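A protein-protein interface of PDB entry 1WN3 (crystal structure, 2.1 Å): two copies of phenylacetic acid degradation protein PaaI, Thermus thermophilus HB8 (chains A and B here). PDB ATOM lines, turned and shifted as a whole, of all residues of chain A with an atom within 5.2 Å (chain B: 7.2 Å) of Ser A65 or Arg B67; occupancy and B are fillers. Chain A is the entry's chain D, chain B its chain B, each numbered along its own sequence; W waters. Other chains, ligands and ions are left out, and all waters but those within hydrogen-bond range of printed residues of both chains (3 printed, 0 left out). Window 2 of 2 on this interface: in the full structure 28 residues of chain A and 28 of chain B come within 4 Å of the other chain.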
ATOM      1  N   ALA A  63      20.495  18.368 -16.764  1.00  0.00           N
ATOM      2  CA  ALA A  63      19.701  19.400 -16.110  1.00  0.00           C
ATOM      3  C   ALA A  63      19.533  19.117 -14.617  1.00  0.00           C
ATOM      4  O   ALA A  63      19.357  17.968 -14.206  1.00  0.00           O
ATOM      5  CB  ALA A  63      18.339  19.501 -16.783  1.00  0.00           C
ATOM      6  N   LEU A  64      19.602  20.172 -13.811  1.00  0.00           N
ATOM      7  CA  LEU A  64      19.449  20.056 -12.366  1.00  0.00           C
ATOM      8  C   LEU A  64      18.171  20.749 -11.901  1.00  0.00           C
ATOM      9  O   LEU A  64      17.264  20.109 -11.374  1.00  0.00           O
ATOM     10  CB  LEU A  64      20.651  20.678 -11.644  1.00  0.00           C
ATOM     11  CG  LEU A  64      22.011  19.978 -11.749  1.00  0.00           C
ATOM     12  CD1 LEU A  64      23.094  20.844 -11.108  1.00  0.00           C
ATOM     13  CD2 LEU A  64      21.934  18.623 -11.063  1.00  0.00           C
ATOM     14  N   SER A  65      18.104  22.061 -12.106  1.00  0.00           N
ATOM     15  CA  SER A  65      16.943  22.839 -11.688  1.00  0.00           C
ATOM     16  C   SER A  65      16.521  23.838 -12.751  1.00  0.00           C
ATOM     17  O   SER A  65      17.349  24.571 -13.295  1.00  0.00           O
ATOM     18  CB  SER A  65      17.254  23.585 -10.391  1.00  0.00           C
ATOM     19  OG  SER A  65      16.143  24.341  -9.952  1.00  0.00           O
ATOM     20  N   CYS A  66      15.223  23.865 -13.039  1.00  0.00           N
ATOM     21  CA  CYS A  66      14.682  24.778 -14.031  1.00  0.00           C
ATOM     22  C   CYS A  66      13.459  25.508 -13.485  1.00  0.00           C
ATOM     23  O   CYS A  66      12.647  24.930 -12.763  1.00  0.00           O
ATOM     24  CB  CYS A  66      14.291  24.013 -15.294  1.00  0.00           C
ATOM     25  SG  CYS A  66      15.649  23.106 -16.010  1.00  0.00           S
ATOM     26  N   ARG A  67      13.342  26.782 -13.830  1.00  0.00           N
ATOM     27  CA  ARG A  67      12.208  27.587 -13.404  1.00  0.00           C
ATOM     28  C   ARG A  67      11.509  28.098 -14.649  1.00  0.00           C
ATOM     29  O   ARG A  67      12.159  28.428 -15.646  1.00  0.00           O
ATOM     30  CB  ARG A  67      12.675  28.772 -12.556  1.00  0.00           C
ATOM     31  CG  ARG A  67      11.578  29.775 -12.197  1.00  0.00           C
ATOM     32  CD  ARG A  67      12.178  31.001 -11.489  1.00  0.00           C
ATOM     33  NE  ARG A  67      11.176  32.021 -11.199  1.00  0.00           N
ATOM     34  CZ  ARG A  67      10.620  32.205 -10.006  1.00  0.00           C
ATOM     35  NH1 ARG A  67      10.974  31.437  -8.984  1.00  0.00           N
ATOM     36  NH2 ARG A  67       9.705  33.150  -9.839  1.00  0.00           N
ATOM     37  N   MET A  68      10.183  28.155 -14.596  1.00  0.00           N
ATOM     38  CA  MET A  68       9.405  28.647 -15.725  1.00  0.00           C
ATOM     39  C   MET A  68       8.382  29.662 -15.245  1.00  0.00           C
ATOM     40  O   MET A  68       7.521  29.339 -14.430  1.00  0.00           O
ATOM     41  CB  MET A  68       8.673  27.497 -16.415  1.00  0.00           C
ATOM     42  CG  MET A  68       7.853  27.928 -17.624  1.00  0.00           C
ATOM     43  SD  MET A  68       8.840  28.147 -19.123  1.00  0.00           S
ATOM     44  CE  MET A  68       7.615  27.818 -20.356  1.00  0.00           C
ATOM     45  N   THR A 111      14.508  29.702 -16.705  1.00  0.00           N
ATOM     46  CA  THR A 111      15.832  29.813 -16.109  1.00  0.00           C
ATOM     47  C   THR A 111      16.221  28.393 -15.735  1.00  0.00           C
ATOM     48  O   THR A 111      15.444  27.686 -15.091  1.00  0.00           O
ATOM     49  CB  THR A 111      15.805  30.671 -14.836  1.00  0.00           C
ATOM     50  OG1 THR A 111      15.144  31.910 -15.107  1.00  0.00           O
ATOM     51  CG2 THR A 111      17.224  30.952 -14.362  1.00  0.00           C
ATOM     52  N   GLY A 112      17.412  27.965 -16.136  1.00  0.00           N
ATOM     53  CA  GLY A 112      17.818  26.607 -15.827  1.00  0.00           C
ATOM     54  C   GLY A 112      19.303  26.419 -15.622  1.00  0.00           C
ATOM     55  O   GLY A 112      20.128  27.131 -16.205  1.00  0.00           O
ATOM     56  N   THR A 113      19.642  25.440 -14.794  1.00  0.00           N
ATOM     57  CA  THR A 113      21.033  25.149 -14.497  1.00  0.00           C
ATOM     58  C   THR A 113      21.317  23.674 -14.711  1.00  0.00           C
ATOM     59  O   THR A 113      20.532  22.813 -14.307  1.00  0.00           O
ATOM     60  CB  THR A 113      21.385  25.511 -13.036  1.00  0.00           C
ATOM     61  OG1 THR A 113      21.303  26.931 -12.859  1.00  0.00           O
ATOM     62  CG2 THR A 113      22.791  25.036 -12.690  1.00  0.00           C
ATOM     63  N   TYR B  44       8.448  17.141 -17.064  1.00  0.00           N
ATOM     64  CA  TYR B  44       7.826  18.380 -16.627  1.00  0.00           C
ATOM     65  C   TYR B  44       6.354  18.411 -17.027  1.00  0.00           C
ATOM     66  O   TYR B  44       5.498  18.798 -16.231  1.00  0.00           O
ATOM     67  CB  TYR B  44       8.536  19.591 -17.238  1.00  0.00           C
ATOM     68  CG  TYR B  44       7.879  20.906 -16.871  1.00  0.00           C
ATOM     69  CD1 TYR B  44       6.765  21.381 -17.571  1.00  0.00           C
ATOM     70  CD2 TYR B  44       8.365  21.668 -15.811  1.00  0.00           C
ATOM     71  CE1 TYR B  44       6.152  22.590 -17.220  1.00  0.00           C
ATOM     72  CE2 TYR B  44       7.766  22.871 -15.453  1.00  0.00           C
ATOM     73  CZ  TYR B  44       6.661  23.329 -16.160  1.00  0.00           C
ATOM     74  OH  TYR B  44       6.081  24.524 -15.789  1.00  0.00           O
ATOM     75  N   ALA B  47       4.345  16.356 -14.588  1.00  0.00           N
ATOM     76  CA  ALA B  47       4.182  17.043 -13.307  1.00  0.00           C
ATOM     77  C   ALA B  47       3.239  18.230 -13.455  1.00  0.00           C
ATOM     78  O   ALA B  47       2.345  18.448 -12.631  1.00  0.00           O
ATOM     79  CB  ALA B  47       5.534  17.522 -12.786  1.00  0.00           C
ATOM     80  N   SER B  65       4.390  30.627 -11.675  1.00  0.00           N
ATOM     81  CA  SER B  65       5.769  30.171 -11.622  1.00  0.00           C
ATOM     82  C   SER B  65       5.865  28.697 -11.209  1.00  0.00           C
ATOM     83  O   SER B  65       5.210  28.229 -10.286  1.00  0.00           O
ATOM     84  CB  SER B  65       6.514  31.047 -10.614  1.00  0.00           C
ATOM     85  OG  SER B  65       7.878  30.625 -10.538  1.00  0.00           O
ATOM     86  N   CYS B  66       6.696  27.946 -11.960  1.00  0.00           N
ATOM     87  CA  CYS B  66       6.924  26.542 -11.618  1.00  0.00           C
ATOM     88  C   CYS B  66       8.417  26.211 -11.563  1.00  0.00           C
ATOM     89  O   CYS B  66       9.227  26.724 -12.324  1.00  0.00           O
ATOM     90  CB  CYS B  66       6.256  25.673 -12.687  1.00  0.00           C
ATOM     91  SG  CYS B  66       4.492  26.017 -12.867  1.00  0.00           S
ATOM     92  N   ARG B  67       8.779  25.346 -10.596  1.00  0.00           N
ATOM     93  CA  ARG B  67      10.159  24.889 -10.519  1.00  0.00           C
ATOM     94  C   ARG B  67      10.240  23.365 -10.669  1.00  0.00           C
ATOM     95  O   ARG B  67       9.441  22.614 -10.132  1.00  0.00           O
ATOM     96  CB  ARG B  67      10.740  25.316  -9.169  1.00  0.00           C
ATOM     97  CG  ARG B  67      12.129  24.726  -8.920  1.00  0.00           C
ATOM     98  CD  ARG B  67      12.733  25.208  -7.598  1.00  0.00           C
ATOM     99  NE  ARG B  67      13.910  24.407  -7.249  1.00  0.00           N
ATOM    100  CZ  ARG B  67      15.090  25.049  -7.165  1.00  0.00           C
ATOM    101  NH1 ARG B  67      15.157  26.349  -7.392  1.00  0.00           N
ATOM    102  NH2 ARG B  67      16.190  24.369  -6.827  1.00  0.00           N
ATOM    103  N   MET B  68      11.226  22.920 -11.465  1.00  0.00           N
ATOM    104  CA  MET B  68      11.425  21.487 -11.639  1.00  0.00           C
ATOM    105  C   MET B  68      12.859  21.081 -11.284  1.00  0.00           C
ATOM    106  O   MET B  68      13.830  21.611 -11.807  1.00  0.00           O
ATOM    107  CB  MET B  68      11.120  21.130 -13.100  1.00  0.00           C
ATOM    108  CG  MET B  68      11.327  19.641 -13.403  1.00  0.00           C
ATOM    109  SD  MET B  68       9.931  18.637 -12.876  1.00  0.00           S
ATOM    110  CE  MET B  68      10.304  17.160 -13.844  1.00  0.00           C
ATOM    111  N   ASP B  69      13.000  20.140 -10.359  1.00  0.00           N
ATOM    112  CA  ASP B  69      14.316  19.657  -9.963  1.00  0.00           C
ATOM    113  C   ASP B  69      14.395  18.194 -10.396  1.00  0.00           C
ATOM    114  O   ASP B  69      13.530  17.401 -10.037  1.00  0.00           O
ATOM    115  CB  ASP B  69      14.502  19.799  -8.444  1.00  0.00           C
ATOM    116  CG  ASP B  69      14.596  21.256  -8.001  1.00  0.00           C
ATOM    117  OD1 ASP B  69      15.475  21.973  -8.529  1.00  0.00           O
ATOM    118  OD2 ASP B  69      13.800  21.690  -7.135  1.00  0.00           O
ATOM    119  N   TYR B  70      15.418  17.855 -11.183  1.00  0.00           N
ATOM    120  CA  TYR B  70      15.611  16.494 -11.703  1.00  0.00           C
ATOM    121  C   TYR B  70      16.606  15.707 -10.857  1.00  0.00           C
ATOM    122  O   TYR B  70      17.713  16.181 -10.603  1.00  0.00           O
ATOM    123  CB  TYR B  70      16.129  16.550 -13.147  1.00  0.00           C
ATOM    124  CG  TYR B  70      15.196  17.238 -14.121  1.00  0.00           C
ATOM    125  CD1 TYR B  70      14.123  16.552 -14.696  1.00  0.00           C
ATOM    126  CD2 TYR B  70      15.370  18.579 -14.450  1.00  0.00           C
ATOM    127  CE1 TYR B  70      13.247  17.191 -15.577  1.00  0.00           C
ATOM    128  CE2 TYR B  70      14.502  19.224 -15.323  1.00  0.00           C
ATOM    129  CZ  TYR B  70      13.442  18.528 -15.885  1.00  0.00           C
ATOM    130  OH  TYR B  70      12.573  19.175 -16.742  1.00  0.00           O
ATOM    131  N   VAL B  98       4.490  18.597  -6.450  1.00  0.00           N
ATOM    132  CA  VAL B  98       4.238  17.460  -7.320  1.00  0.00           C
ATOM    133  C   VAL B  98       5.454  16.547  -7.326  1.00  0.00           C
ATOM    134  O   VAL B  98       6.525  16.918  -7.807  1.00  0.00           O
ATOM    135  CB  VAL B  98       3.933  17.902  -8.779  1.00  0.00           C
ATOM    136  CG1 VAL B  98       3.648  16.681  -9.651  1.00  0.00           C
ATOM    137  CG2 VAL B  98       2.743  18.849  -8.802  1.00  0.00           C
ATOM    138  N   LEU B 109      11.077  16.556  -8.572  1.00  0.00           N
ATOM    139  CA  LEU B 109      10.202  17.306  -7.677  1.00  0.00           C
ATOM    140  C   LEU B 109       9.798  18.595  -8.373  1.00  0.00           C
ATOM    141  O   LEU B 109      10.642  19.328  -8.894  1.00  0.00           O
ATOM    142  CB  LEU B 109      10.908  17.632  -6.362  1.00  0.00           C
ATOM    143  CG  LEU B 109      10.101  18.418  -5.327  1.00  0.00           C
ATOM    144  CD1 LEU B 109       8.867  17.623  -4.892  1.00  0.00           C
ATOM    145  CD2 LEU B 109      10.987  18.717  -4.136  1.00  0.00           C
ATOM    146  N   PHE B 110       8.499  18.861  -8.368  1.00  0.00           N
ATOM    147  CA  PHE B 110       7.938  20.036  -9.014  1.00  0.00           C
ATOM    148  C   PHE B 110       7.187  20.890  -7.997  1.00  0.00           C
ATOM    149  O   PHE B 110       6.510  20.369  -7.116  1.00  0.00           O
ATOM    150  CB  PHE B 110       7.016  19.559 -10.148  1.00  0.00           C
ATOM    151  CG  PHE B 110       6.183  20.640 -10.789  1.00  0.00           C
ATOM    152  CD1 PHE B 110       5.084  21.189 -10.123  1.00  0.00           C
ATOM    153  CD2 PHE B 110       6.436  21.037 -12.099  1.00  0.00           C
ATOM    154  CE1 PHE B 110       4.243  22.111 -10.758  1.00  0.00           C
ATOM    155  CE2 PHE B 110       5.604  21.958 -12.744  1.00  0.00           C
ATOM    156  CZ  PHE B 110       4.504  22.495 -12.072  1.00  0.00           C
ATOM    157  N   THR B 111       7.334  22.204  -8.116  1.00  0.00           N
ATOM    158  CA  THR B 111       6.656  23.149  -7.232  1.00  0.00           C
ATOM    159  C   THR B 111       6.017  24.193  -8.140  1.00  0.00           C
ATOM    160  O   THR B 111       6.696  24.775  -8.984  1.00  0.00           O
ATOM    161  CB  THR B 111       7.642  23.892  -6.309  1.00  0.00           C
ATOM    162  OG1 THR B 111       8.494  22.954  -5.644  1.00  0.00           O
ATOM    163  CG2 THR B 111       6.880  24.708  -5.272  1.00  0.00           C
ATOM    164  N   GLY B 112       4.726  24.440  -7.975  1.00  0.00           N
ATOM    165  CA  GLY B 112       4.086  25.427  -8.823  1.00  0.00           C
ATOM    166  C   GLY B 112       3.060  26.279  -8.108  1.00  0.00           C
ATOM    167  O   GLY B 112       2.370  25.821  -7.204  1.00  0.00           O
ATOM    168  N   THR B 113       2.957  27.532  -8.524  1.00  0.00           N
ATOM    169  CA  THR B 113       1.995  28.449  -7.939  1.00  0.00           C
ATOM    170  C   THR B 113       1.074  28.952  -9.046  1.00  0.00           C
ATOM    171  O   THR B 113       1.515  29.204 -10.170  1.00  0.00           O
ATOM    172  CB  THR B 113       2.712  29.636  -7.260  1.00  0.00           C
ATOM    173  OG1 THR B 113       3.429  29.156  -6.115  1.00  0.00           O
ATOM    174  CG2 THR B 113       1.707  30.706  -6.811  1.00  0.00           C
HETATM  175  O   HOH W   1      18.523  18.153  -8.946  1.00  0.00           O
HETATM  176  O   HOH W   2      17.989  20.750  -8.552  1.00  0.00           O
HETATM  177  O   HOH W   3      19.741  15.820 -12.501  1.00  0.00           O
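The backbone NH (N) of Met A68 is in hydrogen-bond range of the backbone carbonyl oxygen (O) of Cys B66 (2.9 Å). The side-chain hydroxyl (OG) of Ser B65 sits at hydrogen-bond distance from the guanidinium group (NH2) of Arg A67 (3.2 Å). The backbone NH of Met B68 sits at hydrogen-bond distance from the backbone carbonyl oxygen of Cys A66 (2.8 Å). The side-chain hydroxyl of Ser A65 lies close to the guanidinium group of Arg B67 (3.1 Å). OD1 of Asp B69 sits at hydrogen-bond distance from OG of Ser A65 (2.8 Å). The backbone NH (N) of Tyr B70 lies within hydrogen-bond range of the backbone carbonyl oxygen (O) of Leu A64 (2.9 Å).
The backbone carbonyl oxygen of Ser A65 is in hydrogen-bond range of the backbone NH of Thr A113 (2.9 Å). N of Thr B113 is in hydrogen-bond range of O of Ser B65. OD2 of Asp B69 lies within salt-bridge range of NE of Arg B67 (2.7 Å). The backbone carbonyl oxygen (O) of Thr A111 lies within hydrogen-bond range of the backbone NH (N) of Arg A67. The backbone NH (N) of Asp B69 sits at hydrogen-bond distance from the backbone carbonyl oxygen (O) of Leu B109. OH of Tyr B44 lies close to SG of Cys B66 (3.6 Å).
CB of Tyr B70 touches O of Ala A63 (3.7 Å). Leu A64 touches Met B68 (O to O, 3.8 Å). O of Leu A64 touches CA of Asp B69, 3.3 Å away. CA of Ser A65 touches O of Met B68, at 3.3 Å. Cys B66 touches Cys A66. Cys A66 touches Arg B67. Arg A67 touches Cys B66. CB of Met A68 touches OH of Tyr B44, at 3.99 Å. Ser B65 touches Met A68 (CA to O, 3.4 Å).
Of chain B, only Arg B67 (3.1 Å), Met B68 (3.3 Å) and Asp B69 (2.8 Å) come within 4 Å of Ser A65. Arg B67 touches just these residues of chain A: Ser A65 (3.1 Å) and Cys A66 (3.4 Å). Of the printed residues of chain A, Met B68 touches Leu A64 (3.8 Å), Ser A65 (3.3 Å) and Cys A66 (2.8 Å). Printed residues of chain B within 4 Å of Cys A66: Cys B66 (3.9 Å), Arg B67 (3.4 Å) and Met B68 (2.8 Å). Of the printed residues of chain A, Cys B66 touches Cys A66, Arg A67 and Met A68. Thr A111 touches none of the printed residues of chain B. Ala B47 touches none of the printed residues of chain A. The nearest residue of chain B that does not touch Ser A65 is Tyr B70 (5.0 Å). The nearest residue of chain A that does not touch Arg B67 is Arg A67 (4.4 Å).
Of the 14 printed residues of chain B, 7 touch a printed residue of chain A. Printed residues of chain B that touch a printed residue of chain A: Tyr B44, Ser B65, Cys B66, Arg B67, Met B68, Asp B69 and Tyr B70. Hydrophobic or aromatic side chains of chain A that line the printed part of chain B: Ala A63 and Met A68. Among the printed residues, 15 pairs touch across the chains.
Ser A65 touches Met B68, and with the chains exchanged Met A68 touches Ser B65. Cys B66 touches its own counterpart, Cys A66. Cys A66 touches Arg B67, and with the chains exchanged Arg A67 touches Cys B66. Cys A66 touches Met B68, and with the chains exchanged Met A68 touches Cys B66. Positions printed for both chains: 65, 66, 67, 68, 111, 112 and 113. Of the 15 pairs that touch across the chains among the printed residues, 9 have their exchanged pair printed and touching as well.
Water W1 lies within hydrogen-bond range of the backbone carbonyl oxygen (O) of Tyr B70 (2.7 Å) and the backbone carbonyl oxygen (O) of Leu A64 (3.4 Å). Water W3 lies within hydrogen-bond range of the backbone carbonyl oxygen (O) of Ala A63 (2.8 Å) and the backbone carbonyl oxygen (O) of Tyr B70 (2.8 Å). Water W2 lies within hydrogen-bond range of OD1 of Asp B69 (2.8 Å) and O of Leu A64 (3.0 Å).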
